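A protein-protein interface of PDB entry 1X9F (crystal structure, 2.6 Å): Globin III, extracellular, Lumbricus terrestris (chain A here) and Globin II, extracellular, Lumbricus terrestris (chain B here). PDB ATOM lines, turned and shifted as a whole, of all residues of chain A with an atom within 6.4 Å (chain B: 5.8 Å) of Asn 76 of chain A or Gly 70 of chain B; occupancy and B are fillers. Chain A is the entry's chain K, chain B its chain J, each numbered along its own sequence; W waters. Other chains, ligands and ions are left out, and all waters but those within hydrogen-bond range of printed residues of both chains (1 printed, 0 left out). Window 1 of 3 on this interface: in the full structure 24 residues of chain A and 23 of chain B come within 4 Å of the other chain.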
ATOM      1  N   LYS A  32     -15.607  20.259   1.656  1.00  0.00           N
ATOM      2  CA  LYS A  32     -14.242  19.879   1.298  1.00  0.00           C
ATOM      3  C   LYS A  32     -14.220  18.563   0.522  1.00  0.00           C
ATOM      4  O   LYS A  32     -13.610  18.483  -0.558  1.00  0.00           O
ATOM      5  CB  LYS A  32     -13.338  19.819   2.536  1.00  0.00           C
ATOM      6  CG  LYS A  32     -12.771  21.172   2.974  1.00  0.00           C
ATOM      7  CD  LYS A  32     -12.433  21.194   4.467  1.00  0.00           C
ATOM      8  CE  LYS A  32     -11.695  22.478   4.880  1.00  0.00           C
ATOM      9  NZ  LYS A  32     -11.504  22.546   6.378  1.00  0.00           N
ATOM     10  N   ALA A  71      -9.347  13.416   0.032  1.00  0.00           N
ATOM     11  CA  ALA A  71      -9.953  14.638  -0.504  1.00  0.00           C
ATOM     12  C   ALA A  71      -9.820  15.775   0.499  1.00  0.00           C
ATOM     13  O   ALA A  71      -9.522  16.920   0.130  1.00  0.00           O
ATOM     14  CB  ALA A  71     -11.419  14.398  -0.847  1.00  0.00           C
ATOM     15  N   LEU A  72     -10.037  15.448   1.773  1.00  0.00           N
ATOM     16  CA  LEU A  72      -9.822  16.395   2.859  1.00  0.00           C
ATOM     17  C   LEU A  72      -8.358  16.783   2.980  1.00  0.00           C
ATOM     18  O   LEU A  72      -8.048  17.956   3.182  1.00  0.00           O
ATOM     19  CB  LEU A  72     -10.312  15.827   4.194  1.00  0.00           C
ATOM     20  CG  LEU A  72     -11.818  15.615   4.327  1.00  0.00           C
ATOM     21  CD1 LEU A  72     -12.098  14.674   5.481  1.00  0.00           C
ATOM     22  CD2 LEU A  72     -12.548  16.937   4.514  1.00  0.00           C
ATOM     23  N   ARG A  73      -7.461  15.810   2.855  1.00  0.00           N
ATOM     24  CA  ARG A  73      -6.035  16.068   3.042  1.00  0.00           C
ATOM     25  C   ARG A  73      -5.535  17.082   2.013  1.00  0.00           C
ATOM     26  O   ARG A  73      -4.836  18.039   2.363  1.00  0.00           O
ATOM     27  CB  ARG A  73      -5.254  14.760   2.953  1.00  0.00           C
ATOM     28  CG  ARG A  73      -4.292  14.513   4.106  1.00  0.00           C
ATOM     29  CD  ARG A  73      -4.420  13.115   4.707  1.00  0.00           C
ATOM     30  NE  ARG A  73      -4.438  12.067   3.687  1.00  0.00           N
ATOM     31  CZ  ARG A  73      -5.113  10.928   3.784  1.00  0.00           C
ATOM     32  NH1 ARG A  73      -5.853  10.667   4.857  1.00  0.00           N
ATOM     33  NH2 ARG A  73      -5.059  10.047   2.793  1.00  0.00           N
ATOM     34  N   ILE A  74      -5.919  16.876   0.752  1.00  0.00           N
ATOM     35  CA  ILE A  74      -5.582  17.812  -0.320  1.00  0.00           C
ATOM     36  C   ILE A  74      -6.247  19.185  -0.164  1.00  0.00           C
ATOM     37  O   ILE A  74      -5.593  20.214  -0.367  1.00  0.00           O
ATOM     38  CB  ILE A  74      -5.899  17.251  -1.726  1.00  0.00           C
ATOM     39  CG1 ILE A  74      -5.722  18.372  -2.765  1.00  0.00           C
ATOM     40  CG2 ILE A  74      -7.310  16.676  -1.797  1.00  0.00           C
ATOM     41  CD1 ILE A  74      -6.358  18.092  -4.169  1.00  0.00           C
ATOM     42  N   LEU A  75      -7.536  19.206   0.173  1.00  0.00           N
ATOM     43  CA  LEU A  75      -8.225  20.480   0.368  1.00  0.00           C
ATOM     44  C   LEU A  75      -7.595  21.293   1.481  1.00  0.00           C
ATOM     45  O   LEU A  75      -7.446  22.509   1.351  1.00  0.00           O
ATOM     46  CB  LEU A  75      -9.725  20.302   0.623  1.00  0.00           C
ATOM     47  CG  LEU A  75     -10.656  20.967  -0.396  1.00  0.00           C
ATOM     48  CD1 LEU A  75     -10.382  22.472  -0.469  1.00  0.00           C
ATOM     49  CD2 LEU A  75     -10.533  20.349  -1.777  1.00  0.00           C
ATOM     50  N   ASN A  76      -7.220  20.624   2.566  1.00  0.00           N
ATOM     51  CA  ASN A  76      -6.533  21.294   3.662  1.00  0.00           C
ATOM     52  C   ASN A  76      -5.125  21.712   3.291  1.00  0.00           C
ATOM     53  O   ASN A  76      -4.604  22.700   3.811  1.00  0.00           O
ATOM     54  CB  ASN A  76      -6.512  20.401   4.895  1.00  0.00           C
ATOM     55  CG  ASN A  76      -7.698  20.643   5.794  1.00  0.00           C
ATOM     56  OD1 ASN A  76      -8.774  21.040   5.338  1.00  0.00           O
ATOM     57  ND2 ASN A  76      -7.512  20.418   7.090  1.00  0.00           N
ATOM     58  N   GLY A  77      -4.510  20.940   2.398  1.00  0.00           N
ATOM     59  CA  GLY A  77      -3.215  21.287   1.826  1.00  0.00           C
ATOM     60  C   GLY A  77      -3.311  22.618   1.107  1.00  0.00           C
ATOM     61  O   GLY A  77      -2.492  23.516   1.330  1.00  0.00           O
ATOM     62  N   LEU A  78      -4.325  22.745   0.253  1.00  0.00           N
ATOM     63  CA  LEU A  78      -4.579  23.991  -0.456  1.00  0.00           C
ATOM     64  C   LEU A  78      -5.013  25.095   0.510  1.00  0.00           C
ATOM     65  O   LEU A  78      -4.638  26.258   0.336  1.00  0.00           O
ATOM     66  CB  LEU A  78      -5.616  23.786  -1.564  1.00  0.00           C
ATOM     67  CG  LEU A  78      -6.059  25.014  -2.371  1.00  0.00           C
ATOM     68  CD1 LEU A  78      -4.884  25.733  -3.045  1.00  0.00           C
ATOM     69  CD2 LEU A  78      -7.090  24.605  -3.404  1.00  0.00           C
ATOM     70  N   ASP A  79      -5.785  24.729   1.531  1.00  0.00           N
ATOM     71  CA  ASP A  79      -6.202  25.688   2.552  1.00  0.00           C
ATOM     72  C   ASP A  79      -5.016  26.205   3.357  1.00  0.00           C
ATOM     73  O   ASP A  79      -5.009  27.365   3.776  1.00  0.00           O
ATOM     74  CB  ASP A  79      -7.230  25.072   3.501  1.00  0.00           C
ATOM     75  CG  ASP A  79      -7.787  26.080   4.496  1.00  0.00           C
ATOM     76  OD1 ASP A  79      -7.652  25.863   5.718  1.00  0.00           O
ATOM     77  OD2 ASP A  79      -8.378  27.134   4.145  1.00  0.00           O
ATOM     78  N   LEU A  80      -4.031  25.336   3.580  1.00  0.00           N
ATOM     79  CA  LEU A  80      -2.818  25.710   4.301  1.00  0.00           C
ATOM     80  C   LEU A  80      -2.062  26.793   3.539  1.00  0.00           C
ATOM     81  O   LEU A  80      -1.683  27.820   4.113  1.00  0.00           O
ATOM     82  CB  LEU A  80      -1.927  24.482   4.498  1.00  0.00           C
ATOM     83  CG  LEU A  80      -0.514  24.675   5.045  1.00  0.00           C
ATOM     84  CD1 LEU A  80      -0.548  25.041   6.507  1.00  0.00           C
ATOM     85  CD2 LEU A  80       0.289  23.418   4.852  1.00  0.00           C
ATOM     86  N   ALA A  81      -1.861  26.555   2.241  1.00  0.00           N
ATOM     87  CA  ALA A  81      -1.149  27.489   1.373  1.00  0.00           C
ATOM     88  C   ALA A  81      -1.864  28.828   1.301  1.00  0.00           C
ATOM     89  O   ALA A  81      -1.235  29.873   1.503  1.00  0.00           O
ATOM     90  CB  ALA A  81      -0.962  26.903  -0.023  1.00  0.00           C
ATOM     91  N   TYR B  20     -10.316  28.153  15.645  1.00  0.00           N
ATOM     92  CA  TYR B  20      -9.313  27.910  14.609  1.00  0.00           C
ATOM     93  C   TYR B  20      -8.927  29.152  13.791  1.00  0.00           C
ATOM     94  O   TYR B  20      -7.740  29.382  13.550  1.00  0.00           O
ATOM     95  CB  TYR B  20      -9.794  26.781  13.699  1.00  0.00           C
ATOM     96  CG  TYR B  20      -8.780  26.211  12.736  1.00  0.00           C
ATOM     97  CD1 TYR B  20      -9.203  25.659  11.531  1.00  0.00           C
ATOM     98  CD2 TYR B  20      -7.415  26.195  13.025  1.00  0.00           C
ATOM     99  CE1 TYR B  20      -8.302  25.114  10.632  1.00  0.00           C
ATOM    100  CE2 TYR B  20      -6.502  25.651  12.129  1.00  0.00           C
ATOM    101  CZ  TYR B  20      -6.954  25.116  10.936  1.00  0.00           C
ATOM    102  OH  TYR B  20      -6.061  24.575  10.038  1.00  0.00           O
ATOM    103  N   ALA B  65       3.514  23.529  12.331  1.00  0.00           N
ATOM    104  CA  ALA B  65       2.439  23.736  13.301  1.00  0.00           C
ATOM    105  C   ALA B  65       1.086  23.870  12.603  1.00  0.00           C
ATOM    106  O   ALA B  65       0.114  23.232  13.011  1.00  0.00           O
ATOM    107  CB  ALA B  65       2.729  24.949  14.171  1.00  0.00           C
ATOM    108  N   ASP B  66       1.028  24.688  11.550  1.00  0.00           N
ATOM    109  CA  ASP B  66      -0.179  24.794  10.724  1.00  0.00           C
ATOM    110  C   ASP B  66      -0.537  23.422  10.133  1.00  0.00           C
ATOM    111  O   ASP B  66      -1.713  23.075  10.026  1.00  0.00           O
ATOM    112  CB  ASP B  66      -0.001  25.835   9.602  1.00  0.00           C
ATOM    113  CG  ASP B  66      -0.548  27.220   9.970  1.00  0.00           C
ATOM    114  OD1 ASP B  66      -0.988  27.959   9.054  1.00  0.00           O
ATOM    115  OD2 ASP B  66      -0.580  27.659  11.136  1.00  0.00           O
ATOM    116  N   ARG B  67       0.481  22.646   9.772  1.00  0.00           N
ATOM    117  CA  ARG B  67       0.277  21.321   9.190  1.00  0.00           C
ATOM    118  C   ARG B  67      -0.386  20.379  10.204  1.00  0.00           C
ATOM    119  O   ARG B  67      -1.274  19.586   9.858  1.00  0.00           O
ATOM    120  CB  ARG B  67       1.621  20.768   8.721  1.00  0.00           C
ATOM    121  CG  ARG B  67       1.543  19.811   7.560  1.00  0.00           C
ATOM    122  CD  ARG B  67       2.795  19.774   6.694  1.00  0.00           C
ATOM    123  NE  ARG B  67       4.037  19.721   7.472  1.00  0.00           N
ATOM    124  CZ  ARG B  67       5.054  20.573   7.338  1.00  0.00           C
ATOM    125  NH1 ARG B  67       5.005  21.552   6.442  1.00  0.00           N
ATOM    126  NH2 ARG B  67       6.135  20.435   8.099  1.00  0.00           N
ATOM    127  N   VAL B  68       0.045  20.489  11.457  1.00  0.00           N
ATOM    128  CA  VAL B  68      -0.542  19.736  12.562  1.00  0.00           C
ATOM    129  C   VAL B  68      -2.007  20.089  12.774  1.00  0.00           C
ATOM    130  O   VAL B  68      -2.874  19.203  12.822  1.00  0.00           O
ATOM    131  CB  VAL B  68       0.194  20.043  13.865  1.00  0.00           C
ATOM    132  CG1 VAL B  68      -0.535  19.442  15.077  1.00  0.00           C
ATOM    133  CG2 VAL B  68       1.627  19.584  13.762  1.00  0.00           C
ATOM    134  N   LEU B  69      -2.282  21.381  12.931  1.00  0.00           N
ATOM    135  CA  LEU B  69      -3.647  21.842  13.100  1.00  0.00           C
ATOM    136  C   LEU B  69      -4.464  21.476  11.876  1.00  0.00           C
ATOM    137  O   LEU B  69      -5.680  21.316  11.964  1.00  0.00           O
ATOM    138  CB  LEU B  69      -3.696  23.345  13.343  1.00  0.00           C
ATOM    139  CG  LEU B  69      -3.107  23.824  14.670  1.00  0.00           C
ATOM    140  CD1 LEU B  69      -3.678  25.179  14.970  1.00  0.00           C
ATOM    141  CD2 LEU B  69      -3.403  22.866  15.826  1.00  0.00           C
ATOM    142  N   GLY B  70      -3.784  21.329  10.738  1.00  0.00           N
ATOM    143  CA  GLY B  70      -4.443  20.878   9.507  1.00  0.00           C
ATOM    144  C   GLY B  70      -4.990  19.476   9.676  1.00  0.00           C
ATOM    145  O   GLY B  70      -6.117  19.190   9.264  1.00  0.00           O
ATOM    146  N   GLY B  71      -4.184  18.606  10.282  1.00  0.00           N
ATOM    147  CA  GLY B  71      -4.583  17.230  10.565  1.00  0.00           C
ATOM    148  C   GLY B  71      -5.655  17.174  11.636  1.00  0.00           C
ATOM    149  O   GLY B  71      -6.626  16.420  11.516  1.00  0.00           O
ATOM    150  N   LEU B  72      -5.480  17.975  12.682  1.00  0.00           N
ATOM    151  CA  LEU B  72      -6.460  18.027  13.759  1.00  0.00           C
ATOM    152  C   LEU B  72      -7.810  18.465  13.200  1.00  0.00           C
ATOM    153  O   LEU B  72      -8.859  17.949  13.604  1.00  0.00           O
ATOM    154  CB  LEU B  72      -5.999  18.965  14.876  1.00  0.00           C
ATOM    155  CG  LEU B  72      -6.858  19.022  16.144  1.00  0.00           C
ATOM    156  CD1 LEU B  72      -7.081  17.633  16.756  1.00  0.00           C
ATOM    157  CD2 LEU B  72      -6.227  19.960  17.161  1.00  0.00           C
ATOM    158  N   ASP B  73      -7.761  19.399  12.251  1.00  0.00           N
ATOM    159  CA  ASP B  73      -8.952  19.948  11.609  1.00  0.00           C
ATOM    160  C   ASP B  73      -9.763  18.890  10.870  1.00  0.00           C
ATOM    161  O   ASP B  73     -10.989  18.863  10.978  1.00  0.00           O
ATOM    162  CB  ASP B  73      -8.567  21.073  10.648  1.00  0.00           C
ATOM    163  CG  ASP B  73      -9.764  21.678   9.955  1.00  0.00           C
ATOM    164  OD1 ASP B  73      -9.982  21.350   8.769  1.00  0.00           O
ATOM    165  OD2 ASP B  73     -10.550  22.474  10.516  1.00  0.00           O
ATOM    166  N   ILE B  74      -9.076  18.032  10.120  1.00  0.00           N
ATOM    167  CA  ILE B  74      -9.730  16.936   9.416  1.00  0.00           C
ATOM    168  C   ILE B  74     -10.406  16.012  10.429  1.00  0.00           C
ATOM    169  O   ILE B  74     -11.576  15.651  10.269  1.00  0.00           O
ATOM    170  CB  ILE B  74      -8.709  16.140   8.577  1.00  0.00           C
ATOM    171  CG1 ILE B  74      -8.090  17.020   7.486  1.00  0.00           C
ATOM    172  CG2 ILE B  74      -9.371  14.911   7.963  1.00  0.00           C
ATOM    173  CD1 ILE B  74      -6.976  16.321   6.682  1.00  0.00           C
ATOM    174  N   ALA B  75      -9.664  15.641  11.470  1.00  0.00           N
ATOM    175  CA  ALA B  75     -10.174  14.758  12.516  1.00  0.00           C
ATOM    176  C   ALA B  75     -11.424  15.317  13.202  1.00  0.00           C
ATOM    177  O   ALA B  75     -12.465  14.651  13.234  1.00  0.00           O
ATOM    178  CB  ALA B  75      -9.084  14.458  13.540  1.00  0.00           C
HETATM  179  O   HOH W   1      -7.136  23.412   7.519  1.00  0.00           O
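The side-chain amide nitrogen (ND2) of Asn 76 of chain A sits at hydrogen-bond distance from the backbone carbonyl oxygen (O) of Gly 70 of chain B (2.9 Å). The side-chain amide nitrogen (ND2) of Asn 76 of chain A lies within hydrogen-bond range of the side-chain carboxylate (OD1) of Asp 73 of chain B (3.1 Å). OD1 of Asp 73 of chain B is in salt-bridge range of NZ of Lys 32 of chain A, 3.1 Å away.
OD1 of Asn 76 of chain A sits at hydrogen-bond distance from NZ of Lys 32 of chain A (3.3 Å).
CD1 of Leu 72 of chain A touches CG2 of Ile 74 of chain B, at 3.7 Å. CA of Arg 73 of chain A touches CD1 of Ile 74 of chain B (3.8 Å). Ile 74 of chain B touches Asn 76 of chain A (CG1 to ND2, 3.5 Å). Leu 80 of chain A touches Asp 66 of chain B (CD1 to CB, 3.2 Å).
Of the printed residues of chain B, Lys 32 of chain A touches Asp 73. Of the printed residues of chain B, Leu 72 of chain A touches Ile 74. Asn 76 of chain A touches just these residues of chain B: Gly 70, Asp 73 and Ile 74. Asp 79 of chain A touches none of the printed residues of chain B. Printed residues of chain B within 4 Å of Leu 80 of chain A: Asp 66 (3.2 Å). Of the printed residues of chain A, Asp 66 of chain B touches Leu 80 (3.2 Å). Gly 70 of chain B touches just one residue of chain A: Asn 76 (2.9 Å). Leu 72 of chain B touches none of the printed residues of chain A. Printed residues of chain A within 4 Å of Ile 74 of chain B: Leu 72 (3.7 Å), Arg 73 (3.8 Å) and Asn 76 (3.5 Å). The nearest residue of chain B that does not touch Asn 76 of chain A is Gly 71 of chain B (5.0 Å). The nearest printed residue of chain A that does not touch Gly 70 of chain B is Leu 80 of chain A (6.4 Å).
Of the 12 printed residues of chain A, 5 touch a printed residue of chain B. Printed residues of chain A that touch a printed residue of chain B: Lys 32, Leu 72, Arg 73, Asn 76 and Leu 80. Among the printed residues, 7 pairs touch across the chains.
Water W1 lies within hydrogen-bond range of OH of Tyr 20 of chain B, ND2 of Asn 76 of chain A and OD1 of Asp 79 of chain A.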
